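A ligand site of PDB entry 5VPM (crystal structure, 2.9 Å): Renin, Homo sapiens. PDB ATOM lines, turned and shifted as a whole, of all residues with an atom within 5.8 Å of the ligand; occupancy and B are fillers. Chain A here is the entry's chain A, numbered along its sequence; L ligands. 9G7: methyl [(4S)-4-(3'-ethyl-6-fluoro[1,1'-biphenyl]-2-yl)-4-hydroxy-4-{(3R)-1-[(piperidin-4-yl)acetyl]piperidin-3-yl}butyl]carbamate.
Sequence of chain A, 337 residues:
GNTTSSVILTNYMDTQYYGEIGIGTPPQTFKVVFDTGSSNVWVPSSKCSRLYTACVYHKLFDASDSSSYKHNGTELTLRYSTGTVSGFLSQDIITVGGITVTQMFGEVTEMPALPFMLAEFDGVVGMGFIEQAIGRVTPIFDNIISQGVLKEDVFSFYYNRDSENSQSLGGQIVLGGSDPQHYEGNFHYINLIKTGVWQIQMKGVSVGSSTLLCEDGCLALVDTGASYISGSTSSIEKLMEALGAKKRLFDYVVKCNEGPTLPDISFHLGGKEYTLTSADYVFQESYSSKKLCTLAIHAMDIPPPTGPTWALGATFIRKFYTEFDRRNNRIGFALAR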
ATOM      1  N   THR A  15      17.842   4.387  -5.937  1.00  0.00           N
ATOM      2  CA  THR A  15      18.514   4.230  -7.221  1.00  0.00           C
ATOM      3  C   THR A  15      18.262   2.879  -7.856  1.00  0.00           C
ATOM      4  O   THR A  15      18.235   2.784  -9.078  1.00  0.00           O
ATOM      5  CB  THR A  15      20.004   4.492  -7.027  1.00  0.00           C
ATOM      6  OG1 THR A  15      20.174   5.880  -6.796  1.00  0.00           O
ATOM      7  CG2 THR A  15      20.821   4.129  -8.244  1.00  0.00           C
ATOM      8  N   GLN A  16      18.081   1.834  -7.046  1.00  0.00           N
ATOM      9  CA  GLN A  16      17.723   0.509  -7.548  1.00  0.00           C
ATOM     10  C   GLN A  16      16.472   0.011  -6.838  1.00  0.00           C
ATOM     11  O   GLN A  16      16.465  -0.071  -5.606  1.00  0.00           O
ATOM     12  CB  GLN A  16      18.874  -0.476  -7.354  1.00  0.00           C
ATOM     13  CG  GLN A  16      20.249   0.180  -7.506  1.00  0.00           C
ATOM     14  CD  GLN A  16      21.369  -0.819  -7.602  1.00  0.00           C
ATOM     15  OE1 GLN A  16      21.139  -2.036  -7.611  1.00  0.00           O
ATOM     16  NE2 GLN A  16      22.595  -0.322  -7.683  1.00  0.00           N
ATOM     17  N   TYR A  17      15.432  -0.309  -7.602  1.00  0.00           N
ATOM     18  CA  TYR A  17      14.229  -0.942  -7.077  1.00  0.00           C
ATOM     19  C   TYR A  17      14.107  -2.335  -7.711  1.00  0.00           C
ATOM     20  O   TYR A  17      13.870  -2.459  -8.929  1.00  0.00           O
ATOM     21  CB  TYR A  17      12.982  -0.093  -7.389  1.00  0.00           C
ATOM     22  CG  TYR A  17      12.938   1.271  -6.724  1.00  0.00           C
ATOM     23  CD1 TYR A  17      13.640   2.340  -7.250  1.00  0.00           C
ATOM     24  CD2 TYR A  17      12.184   1.486  -5.581  1.00  0.00           C
ATOM     25  CE1 TYR A  17      13.610   3.597  -6.656  1.00  0.00           C
ATOM     26  CE2 TYR A  17      12.137   2.742  -4.989  1.00  0.00           C
ATOM     27  CZ  TYR A  17      12.848   3.788  -5.533  1.00  0.00           C
ATOM     28  OH  TYR A  17      12.834   5.037  -4.971  1.00  0.00           O
ATOM     29  N   TYR A  18      14.268  -3.375  -6.890  1.00  0.00           N
ATOM     30  CA  TYR A  18      14.235  -4.777  -7.353  1.00  0.00           C
ATOM     31  C   TYR A  18      13.360  -5.652  -6.465  1.00  0.00           C
ATOM     32  O   TYR A  18      13.170  -5.350  -5.291  1.00  0.00           O
ATOM     33  CB  TYR A  18      15.640  -5.392  -7.436  1.00  0.00           C
ATOM     34  CG  TYR A  18      16.501  -5.225  -6.195  1.00  0.00           C
ATOM     35  CD1 TYR A  18      16.485  -6.172  -5.159  1.00  0.00           C
ATOM     36  CD2 TYR A  18      17.336  -4.134  -6.059  1.00  0.00           C
ATOM     37  CE1 TYR A  18      17.289  -6.018  -4.011  1.00  0.00           C
ATOM     38  CE2 TYR A  18      18.130  -3.967  -4.928  1.00  0.00           C
ATOM     39  CZ  TYR A  18      18.115  -4.902  -3.900  1.00  0.00           C
ATOM     40  OH  TYR A  18      18.922  -4.680  -2.803  1.00  0.00           O
ATOM     41  N   VAL A  33      15.235  -6.181 -11.629  1.00  0.00           N
ATOM     42  CA  VAL A  33      14.642  -4.885 -11.908  1.00  0.00           C
ATOM     43  C   VAL A  33      13.531  -5.075 -12.928  1.00  0.00           C
ATOM     44  O   VAL A  33      13.756  -5.687 -13.957  1.00  0.00           O
ATOM     45  CB  VAL A  33      15.657  -3.885 -12.490  1.00  0.00           C
ATOM     46  CG1 VAL A  33      14.992  -2.550 -12.805  1.00  0.00           C
ATOM     47  CG2 VAL A  33      16.828  -3.689 -11.527  1.00  0.00           C
ATOM     48  N   ASP A  35      11.290  -3.369 -15.684  1.00  0.00           N
ATOM     49  CA  ASP A  35      11.780  -2.294 -16.549  1.00  0.00           C
ATOM     50  C   ASP A  35      10.852  -2.026 -17.724  1.00  0.00           C
ATOM     51  O   ASP A  35      10.888  -2.755 -18.699  1.00  0.00           O
ATOM     52  CB  ASP A  35      13.157  -2.733 -17.046  1.00  0.00           C
ATOM     53  CG  ASP A  35      13.773  -1.782 -18.030  1.00  0.00           C
ATOM     54  OD1 ASP A  35      13.404  -0.594 -18.070  1.00  0.00           O
ATOM     55  OD2 ASP A  35      14.686  -2.240 -18.754  1.00  0.00           O
ATOM     56  N   GLY A  37      11.177   0.253 -19.790  1.00  0.00           N
ATOM     57  CA  GLY A  37      12.050   0.662 -20.872  1.00  0.00           C
ATOM     58  C   GLY A  37      12.646  -0.462 -21.693  1.00  0.00           C
ATOM     59  O   GLY A  37      13.347  -0.183 -22.667  1.00  0.00           O
ATOM     60  N   SER A  38      12.438  -1.715 -21.314  1.00  0.00           N
ATOM     61  CA  SER A  38      12.954  -2.840 -22.095  1.00  0.00           C
ATOM     62  C   SER A  38      11.921  -3.957 -22.140  1.00  0.00           C
ATOM     63  O   SER A  38      10.881  -3.866 -21.489  1.00  0.00           O
ATOM     64  CB  SER A  38      14.313  -3.324 -21.561  1.00  0.00           C
ATOM     65  OG  SER A  38      14.205  -4.031 -20.344  1.00  0.00           O
ATOM     66  N   TRP A  42      16.339 -11.319 -18.460  1.00  0.00           N
ATOM     67  CA  TRP A  42      17.582 -12.062 -18.290  1.00  0.00           C
ATOM     68  C   TRP A  42      18.031 -12.147 -16.852  1.00  0.00           C
ATOM     69  O   TRP A  42      17.671 -11.324 -16.011  1.00  0.00           O
ATOM     70  CB  TRP A  42      18.698 -11.483 -19.152  1.00  0.00           C
ATOM     71  CG  TRP A  42      19.064 -10.078 -18.824  1.00  0.00           C
ATOM     72  CD1 TRP A  42      18.554  -8.946 -19.373  1.00  0.00           C
ATOM     73  CD2 TRP A  42      20.040  -9.660 -17.865  1.00  0.00           C
ATOM     74  NE1 TRP A  42      19.146  -7.839 -18.811  1.00  0.00           N
ATOM     75  CE2 TRP A  42      20.061  -8.250 -17.886  1.00  0.00           C
ATOM     76  CE3 TRP A  42      20.890 -10.335 -16.988  1.00  0.00           C
ATOM     77  CZ2 TRP A  42      20.907  -7.504 -17.065  1.00  0.00           C
ATOM     78  CZ3 TRP A  42      21.741  -9.583 -16.160  1.00  0.00           C
ATOM     79  CH2 TRP A  42      21.737  -8.186 -16.212  1.00  0.00           C
ATOM     80  N   TYR A  80      22.533  -1.542 -23.447  1.00  0.00           N
ATOM     81  CA  TYR A  80      22.119  -0.476 -22.536  1.00  0.00           C
ATOM     82  C   TYR A  80      23.118   0.663 -22.735  1.00  0.00           C
ATOM     83  O   TYR A  80      24.165   0.479 -23.367  1.00  0.00           O
ATOM     84  CB  TYR A  80      22.124  -0.939 -21.068  1.00  0.00           C
ATOM     85  CG  TYR A  80      21.130  -2.045 -20.743  1.00  0.00           C
ATOM     86  CD1 TYR A  80      19.754  -1.801 -20.775  1.00  0.00           C
ATOM     87  CD2 TYR A  80      21.565  -3.335 -20.422  1.00  0.00           C
ATOM     88  CE1 TYR A  80      18.819  -2.808 -20.490  1.00  0.00           C
ATOM     89  CE2 TYR A  80      20.644  -4.359 -20.147  1.00  0.00           C
ATOM     90  CZ  TYR A  80      19.274  -4.100 -20.180  1.00  0.00           C
ATOM     91  OH  TYR A  80      18.358  -5.108 -19.907  1.00  0.00           O
ATOM     92  N   SER A  81      22.807   1.836 -22.191  1.00  0.00           N
ATOM     93  CA  SER A  81      23.694   3.012 -22.302  1.00  0.00           C
ATOM     94  C   SER A  81      25.105   2.809 -21.710  1.00  0.00           C
ATOM     95  O   SER A  81      26.061   3.469 -22.136  1.00  0.00           O
ATOM     96  CB  SER A  81      23.020   4.261 -21.687  1.00  0.00           C
ATOM     97  OG  SER A  81      22.722   4.097 -20.305  1.00  0.00           O
ATOM     98  N   THR A  82      25.212   1.902 -20.741  1.00  0.00           N
ATOM     99  CA  THR A  82      26.474   1.551 -20.085  1.00  0.00           C
ATOM    100  C   THR A  82      27.093   0.268 -20.668  1.00  0.00           C
ATOM    101  O   THR A  82      27.543  -0.622 -19.920  1.00  0.00           O
ATOM    102  CB  THR A  82      26.241   1.377 -18.571  1.00  0.00           C
ATOM    103  OG1 THR A  82      25.090   0.542 -18.380  1.00  0.00           O
ATOM    104  CG2 THR A  82      26.000   2.707 -17.907  1.00  0.00           C
ATOM    105  N   PRO A 115      28.467  -1.769 -15.608  1.00  0.00           N
ATOM    106  CA  PRO A 115      28.075  -1.186 -14.325  1.00  0.00           C
ATOM    107  C   PRO A 115      27.791  -2.159 -13.193  1.00  0.00           C
ATOM    108  O   PRO A 115      27.489  -1.718 -12.103  1.00  0.00           O
ATOM    109  CB  PRO A 115      26.777  -0.477 -14.685  1.00  0.00           C
ATOM    110  CG  PRO A 115      26.161  -1.363 -15.709  1.00  0.00           C
ATOM    111  CD  PRO A 115      27.311  -1.881 -16.530  1.00  0.00           C
ATOM    112  N   PHE A 116      27.887  -3.464 -13.434  1.00  0.00           N
ATOM    113  CA  PHE A 116      27.184  -4.433 -12.575  1.00  0.00           C
ATOM    114  C   PHE A 116      27.803  -4.818 -11.227  1.00  0.00           C
ATOM    115  O   PHE A 116      27.100  -5.413 -10.401  1.00  0.00           O
ATOM    116  CB  PHE A 116      26.837  -5.686 -13.359  1.00  0.00           C
ATOM    117  CG  PHE A 116      25.877  -5.426 -14.465  1.00  0.00           C
ATOM    118  CD1 PHE A 116      24.542  -5.184 -14.189  1.00  0.00           C
ATOM    119  CD2 PHE A 116      26.311  -5.375 -15.785  1.00  0.00           C
ATOM    120  CE1 PHE A 116      23.646  -4.908 -15.209  1.00  0.00           C
ATOM    121  CE2 PHE A 116      25.409  -5.115 -16.804  1.00  0.00           C
ATOM    122  CZ  PHE A 116      24.074  -4.884 -16.519  1.00  0.00           C
ATOM    123  N   LEU A 118      28.284  -2.603  -9.064  1.00  0.00           N
ATOM    124  CA  LEU A 118      27.465  -1.750  -8.197  1.00  0.00           C
ATOM    125  C   LEU A 118      25.991  -2.178  -8.116  1.00  0.00           C
ATOM    126  O   LEU A 118      25.206  -1.537  -7.397  1.00  0.00           O
ATOM    127  CB  LEU A 118      27.545  -0.299  -8.676  1.00  0.00           C
ATOM    128  CG  LEU A 118      28.920   0.360  -8.484  1.00  0.00           C
ATOM    129  CD1 LEU A 118      29.887   0.099  -9.635  1.00  0.00           C
ATOM    130  CD2 LEU A 118      28.738   1.860  -8.271  1.00  0.00           C
ATOM    131  N   ALA A 119      25.619  -3.264  -8.808  1.00  0.00           N
ATOM    132  CA  ALA A 119      24.224  -3.676  -8.969  1.00  0.00           C
ATOM    133  C   ALA A 119      23.789  -4.648  -7.894  1.00  0.00           C
ATOM    134  O   ALA A 119      24.261  -5.772  -7.854  1.00  0.00           O
ATOM    135  CB  ALA A 119      24.039  -4.328 -10.330  1.00  0.00           C
ATOM    136  N   GLU A 120      22.866  -4.231  -7.036  1.00  0.00           N
ATOM    137  CA  GLU A 120      22.280  -5.095  -5.995  1.00  0.00           C
ATOM    138  C   GLU A 120      21.304  -6.128  -6.582  1.00  0.00           C
ATOM    139  O   GLU A 120      21.012  -7.146  -5.956  1.00  0.00           O
ATOM    140  CB  GLU A 120      21.532  -4.252  -4.959  1.00  0.00           C
ATOM    141  CG  GLU A 120      22.332  -3.144  -4.297  1.00  0.00           C
ATOM    142  CD  GLU A 120      23.374  -3.642  -3.337  1.00  0.00           C
ATOM    143  OE1 GLU A 120      23.060  -4.568  -2.567  1.00  0.00           O
ATOM    144  OE2 GLU A 120      24.481  -3.088  -3.326  1.00  0.00           O
ATOM    145  N   PHE A 121      20.777  -5.838  -7.755  1.00  0.00           N
ATOM    146  CA  PHE A 121      19.959  -6.778  -8.512  1.00  0.00           C
ATOM    147  C   PHE A 121      20.846  -7.757  -9.319  1.00  0.00           C
ATOM    148  O   PHE A 121      21.978  -7.437  -9.700  1.00  0.00           O
ATOM    149  CB  PHE A 121      19.053  -6.025  -9.478  1.00  0.00           C
ATOM    150  CG  PHE A 121      19.798  -5.308 -10.573  1.00  0.00           C
ATOM    151  CD1 PHE A 121      20.116  -5.987 -11.754  1.00  0.00           C
ATOM    152  CD2 PHE A 121      20.219  -3.989 -10.414  1.00  0.00           C
ATOM    153  CE1 PHE A 121      20.822  -5.352 -12.750  1.00  0.00           C
ATOM    154  CE2 PHE A 121      20.920  -3.360 -11.417  1.00  0.00           C
ATOM    155  CZ  PHE A 121      21.225  -4.045 -12.585  1.00  0.00           C
ATOM    156  N   VAL A 124      16.937  -8.588 -14.864  1.00  0.00           N
ATOM    157  CA  VAL A 124      15.955  -7.600 -15.323  1.00  0.00           C
ATOM    158  C   VAL A 124      14.774  -8.327 -15.955  1.00  0.00           C
ATOM    159  O   VAL A 124      14.944  -9.366 -16.615  1.00  0.00           O
ATOM    160  CB  VAL A 124      16.564  -6.614 -16.355  1.00  0.00           C
ATOM    161  CG1 VAL A 124      15.541  -5.562 -16.791  1.00  0.00           C
ATOM    162  CG2 VAL A 124      17.816  -5.954 -15.805  1.00  0.00           C
ATOM    163  N   TYR A 159       6.940   3.204  -6.075  1.00  0.00           N
ATOM    164  CA  TYR A 159       8.262   3.411  -5.510  1.00  0.00           C
ATOM    165  C   TYR A 159       8.149   4.346  -4.326  1.00  0.00           C
ATOM    166  O   TYR A 159       7.524   5.418  -4.423  1.00  0.00           O
ATOM    167  CB  TYR A 159       9.207   4.013  -6.541  1.00  0.00           C
ATOM    168  CG  TYR A 159       9.593   3.102  -7.684  1.00  0.00           C
ATOM    169  CD1 TYR A 159       9.646   1.715  -7.532  1.00  0.00           C
ATOM    170  CD2 TYR A 159       9.977   3.647  -8.907  1.00  0.00           C
ATOM    171  CE1 TYR A 159      10.039   0.895  -8.577  1.00  0.00           C
ATOM    172  CE2 TYR A 159      10.370   2.838  -9.961  1.00  0.00           C
ATOM    173  CZ  TYR A 159      10.397   1.461  -9.785  1.00  0.00           C
ATOM    174  OH  TYR A 159      10.782   0.662 -10.827  1.00  0.00           O
ATOM    175  N   ASP A 223       9.691   5.104 -17.707  1.00  0.00           N
ATOM    176  CA  ASP A 223      10.732   4.066 -17.543  1.00  0.00           C
ATOM    177  C   ASP A 223      10.949   3.607 -16.090  1.00  0.00           C
ATOM    178  O   ASP A 223      11.719   4.202 -15.347  1.00  0.00           O
ATOM    179  CB  ASP A 223      12.042   4.631 -18.103  1.00  0.00           C
ATOM    180  CG  ASP A 223      13.103   3.578 -18.358  1.00  0.00           C
ATOM    181  OD1 ASP A 223      12.985   2.432 -17.865  1.00  0.00           O
ATOM    182  OD2 ASP A 223      14.076   3.916 -19.080  1.00  0.00           O
ATOM    183  N   THR A 224      10.314   2.505 -15.709  1.00  0.00           N
ATOM    184  CA  THR A 224      10.484   1.950 -14.350  1.00  0.00           C
ATOM    185  C   THR A 224      11.909   1.451 -14.043  1.00  0.00           C
ATOM    186  O   THR A 224      12.269   1.311 -12.883  1.00  0.00           O
ATOM    187  CB  THR A 224       9.480   0.800 -14.072  1.00  0.00           C
ATOM    188  OG1 THR A 224       9.600  -0.237 -15.062  1.00  0.00           O
ATOM    189  CG2 THR A 224       8.053   1.364 -14.035  1.00  0.00           C
ATOM    190  N   GLY A 225      12.705   1.175 -15.086  1.00  0.00           N
ATOM    191  CA  GLY A 225      14.105   0.800 -14.934  1.00  0.00           C
ATOM    192  C   GLY A 225      15.094   1.933 -14.788  1.00  0.00           C
ATOM    193  O   GLY A 225      16.266   1.688 -14.540  1.00  0.00           O
ATOM    194  N   ALA A 226      14.638   3.172 -14.933  1.00  0.00           N
ATOM    195  CA  ALA A 226      15.509   4.323 -14.821  1.00  0.00           C
ATOM    196  C   ALA A 226      15.512   4.869 -13.378  1.00  0.00           C
ATOM    197  O   ALA A 226      14.459   4.957 -12.757  1.00  0.00           O
ATOM    198  CB  ALA A 226      15.045   5.405 -15.796  1.00  0.00           C
ATOM    199  N   SER A 227      16.689   5.234 -12.874  1.00  0.00           N
ATOM    200  CA  SER A 227      16.831   5.790 -11.515  1.00  0.00           C
ATOM    201  C   SER A 227      16.496   7.266 -11.464  1.00  0.00           C
ATOM    202  O   SER A 227      15.958   7.765 -10.457  1.00  0.00           O
ATOM    203  CB  SER A 227      18.267   5.627 -10.996  1.00  0.00           C
ATOM    204  OG  SER A 227      18.704   4.274 -11.062  1.00  0.00           O
ATOM    205  N   TYR A 228      16.882   7.975 -12.528  1.00  0.00           N
ATOM    206  CA  TYR A 228      16.788   9.435 -12.622  1.00  0.00           C
ATOM    207  C   TYR A 228      15.868   9.819 -13.760  1.00  0.00           C
ATOM    208  O   TYR A 228      15.668   9.036 -14.696  1.00  0.00           O
ATOM    209  CB  TYR A 228      18.173  10.027 -12.916  1.00  0.00           C
ATOM    210  CG  TYR A 228      19.228   9.980 -11.802  1.00  0.00           C
ATOM    211  CD1 TYR A 228      19.017   9.280 -10.607  1.00  0.00           C
ATOM    212  CD2 TYR A 228      20.433  10.649 -11.951  1.00  0.00           C
ATOM    213  CE1 TYR A 228      19.977   9.249  -9.609  1.00  0.00           C
ATOM    214  CE2 TYR A 228      21.405  10.614 -10.957  1.00  0.00           C
ATOM    215  CZ  TYR A 228      21.168   9.914  -9.788  1.00  0.00           C
ATOM    216  OH  TYR A 228      22.116   9.874  -8.790  1.00  0.00           O
ATOM    217  N   HIS A 298      19.515  13.850 -15.079  1.00  0.00           N
ATOM    218  CA  HIS A 298      20.729  13.936 -15.916  1.00  0.00           C
ATOM    219  C   HIS A 298      20.434  13.869 -17.415  1.00  0.00           C
ATOM    220  O   HIS A 298      19.312  13.651 -17.850  1.00  0.00           O
ATOM    221  CB  HIS A 298      21.749  12.856 -15.540  1.00  0.00           C
ATOM    222  CG  HIS A 298      21.405  11.476 -15.998  1.00  0.00           C
ATOM    223  ND1 HIS A 298      20.104  11.033 -16.157  1.00  0.00           N
ATOM    224  CD2 HIS A 298      22.188  10.417 -16.305  1.00  0.00           C
ATOM    225  CE1 HIS A 298      20.108   9.776 -16.553  1.00  0.00           C
ATOM    226  NE2 HIS A 298      21.361   9.374 -16.648  1.00  0.00           N
ATOM    227  N   MET A 300      20.573  12.324 -21.086  1.00  0.00           N
ATOM    228  CA  MET A 300      20.811  11.235 -22.018  1.00  0.00           C
ATOM    229  C   MET A 300      20.066  11.396 -23.320  1.00  0.00           C
ATOM    230  O   MET A 300      18.861  11.555 -23.332  1.00  0.00           O
ATOM    231  CB  MET A 300      20.497   9.886 -21.433  1.00  0.00           C
ATOM    232  CG  MET A 300      21.203   8.791 -22.206  1.00  0.00           C
ATOM    233  SD  MET A 300      21.458   7.327 -21.212  1.00  0.00           S
ATOM    234  CE  MET A 300      22.376   8.029 -19.822  1.00  0.00           C
ATOM    235  N   ALA A 314      12.539   6.819 -11.814  1.00  0.00           N
ATOM    236  CA  ALA A 314      12.156   6.660 -10.408  1.00  0.00           C
ATOM    237  C   ALA A 314      11.934   8.011  -9.715  1.00  0.00           C
ATOM    238  O   ALA A 314      10.961   8.162  -8.969  1.00  0.00           O
ATOM    239  CB  ALA A 314      13.200   5.832  -9.673  1.00  0.00           C
HETATM  240  C10 9G7 L   1      23.598  -0.973 -12.570  1.00  0.00           C
HETATM  241  C13 9G7 L   1      23.842   0.351 -10.631  1.00  0.00           C
HETATM  242  C15 9G7 L   1      22.246   1.000 -12.340  1.00  0.00           C
HETATM  243  C20 9G7 L   1      18.098  -0.301 -11.955  1.00  0.00           C
HETATM  244  C22 9G7 L   1      16.129   0.989 -11.293  1.00  0.00           C
HETATM  245  C26 9G7 L   1      21.623   2.839 -14.100  1.00  0.00           C
HETATM  246  C28 9G7 L   1      23.013   3.451 -14.051  1.00  0.00           C
HETATM  247  C01 9G7 L   1      17.871  -1.924 -15.653  1.00  0.00           C
HETATM  248  C02 9G7 L   1      19.181  -2.652 -15.857  1.00  0.00           C
HETATM  249  C03 9G7 L   1      20.428  -1.759 -15.776  1.00  0.00           C
HETATM  250  C04 9G7 L   1      21.071  -1.349 -16.933  1.00  0.00           C
HETATM  251  C05 9G7 L   1      22.201  -0.547 -16.864  1.00  0.00           C
HETATM  252  C06 9G7 L   1      22.703  -0.154 -15.622  1.00  0.00           C
HETATM  253  C07 9G7 L   1      22.062  -0.533 -14.447  1.00  0.00           C
HETATM  254  C08 9G7 L   1      20.936  -1.363 -14.541  1.00  0.00           C
HETATM  255  C09 9G7 L   1      22.626  -0.146 -13.102  1.00  0.00           C
HETATM  256  F11 9G7 L   1      23.970  -2.064 -13.282  1.00  0.00           F
HETATM  257  C12 9G7 L   1      24.217  -0.755 -11.362  1.00  0.00           C
HETATM  258  C14 9G7 L   1      22.873   1.218 -11.109  1.00  0.00           C
HETATM  259  C16 9G7 L   1      21.162   1.996 -12.821  1.00  0.00           C
HETATM  260  O17 9G7 L   1      21.130   3.085 -11.897  1.00  0.00           O
HETATM  261  C18 9G7 L   1      19.729   1.392 -12.863  1.00  0.00           C
HETATM  262  C19 9G7 L   1      19.328   0.522 -11.674  1.00  0.00           C
HETATM  263  N21 9G7 L   1      16.927   0.518 -12.254  1.00  0.00           N
HETATM  264  O23 9G7 L   1      16.100   0.566 -10.151  1.00  0.00           O
HETATM  265  O24 9G7 L   1      15.361   1.987 -11.745  1.00  0.00           O
HETATM  266  C25 9G7 L   1      14.356   2.485 -10.823  1.00  0.00           C
HETATM  267  C29 9G7 L   1      23.378   4.108 -15.384  1.00  0.00           C
HETATM  268  C30 9G7 L   1      22.346   5.147 -15.792  1.00  0.00           C
HETATM  269  N31 9G7 L   1      20.948   4.578 -15.797  1.00  0.00           N
HETATM  270  C32 9G7 L   1      20.656   4.057 -14.442  1.00  0.00           C
HETATM  271  C33 9G7 L   1      20.137   4.595 -16.896  1.00  0.00           C
HETATM  272  O34 9G7 L   1      20.514   5.081 -17.962  1.00  0.00           O
HETATM  273  C35 9G7 L   1      18.726   4.025 -16.810  1.00  0.00           C
HETATM  274  C36 9G7 L   1      18.361   2.987 -17.874  1.00  0.00           C
HETATM  275  C37 9G7 L   1      18.799   1.594 -17.453  1.00  0.00           C
HETATM  276  C38 9G7 L   1      18.239   0.498 -18.350  1.00  0.00           C
HETATM  277  N39 9G7 L   1      16.770   0.575 -18.409  1.00  0.00           N
HETATM  278  C40 9G7 L   1      16.363   1.785 -19.012  1.00  0.00           C
HETATM  279  C41 9G7 L   1      16.842   2.989 -18.154  1.00  0.00           C
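The backbone NH (N) of Ala 226 lies close to an oxygen (O24) of the ligand (3.5 Å).
The backbone carbonyl oxygen (O) of Gly 225 sits at hydrogen-bond distance from a nitrogen (N21) of the ligand (2.7 Å).
OG of Ser 81 lies within hydrogen-bond range of O34 of the ligand.
OD2 of Asp 35 is in salt-bridge range of N39 of the ligand, 3.5 Å away.
N of Tyr 17 lies within hydrogen-bond range of O23 of the ligand (2.8 Å).
The side-chain hydroxyl of Ser 227 lies within hydrogen-bond range of an oxygen (O17) of the ligand.
N of Glu 120 sits at hydrogen-bond distance from OE1 of Gln 16, 2.9 Å away.
O of Thr 224 lies within hydrogen-bond range of OH of Tyr 159.
OG of Ser 38 is in hydrogen-bond range of OD2 of Asp 35, 2.4 Å away.
The backbone carbonyl oxygen (O) of Val 124 sits at hydrogen-bond distance from the backbone NH (N) of Trp 42, 3.0 Å away.
The side-chain amide nitrogen (NE2) of Gln 16 lies within hydrogen-bond range of the backbone carbonyl oxygen (O) of Leu 118, at 2.9 Å.
OG of Ser 227 sits at hydrogen-bond distance from O of Thr 15, at 2.5 Å.
The backbone NH of Gly 37 is in hydrogen-bond range of the side-chain carboxylate of Asp 223, 3.4 Å away.
The side-chain carboxylate of Asp 223 sits at hydrogen-bond distance from the backbone NH of Gly 225, at 3.1 Å.
O of Thr 15 sits close to O23 of the ligand (3.3 Å).
O of Thr 224 lies close to O24 of the ligand, 3.4 Å away.
Gln 16 touches the ligand (CA to O23, 3.1 Å).
Val 33 touches the ligand (CG2 to C20, 3.6 Å).
Tyr 80 touches the ligand.
OG1 of Thr 82 touches C05 of the ligand, 3.4 Å away.
Pro 115 touches the ligand (CG to F11, 3.3 Å).
CD1 of Phe 116 touches F11 of the ligand, 3.3 Å away.
Leu 118 touches the ligand.
CB of Ala 119 touches F11 of the ligand, at 3.7 Å.
CZ of Phe 121 touches C08 of the ligand, at 3.3 Å.
Val 124 touches the ligand (CG2 to C02, 3.6 Å).
OD2 of Asp 223 touches C41 of the ligand, 3.1 Å away.
CE of Met 300 touches O34 of the ligand, 3.95 Å away.
Ala 314 touches the ligand.
Hydrophobic or aromatic side chains within 4 Å of the ligand: Tyr 17, Val 33, Tyr 80, Pro 115, Phe 116, Ala 119, Phe 121, Val 124, Ala 226, Met 300 and Ala 314.
Of the 29 residues printed, 21 come within 4 Å of the ligand.
Along chain A the residues within 4 Å of the ligand span positions 15 to 314.
The nearest printed residue that does not touch the ligand is Tyr 159 (4.01 Å).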
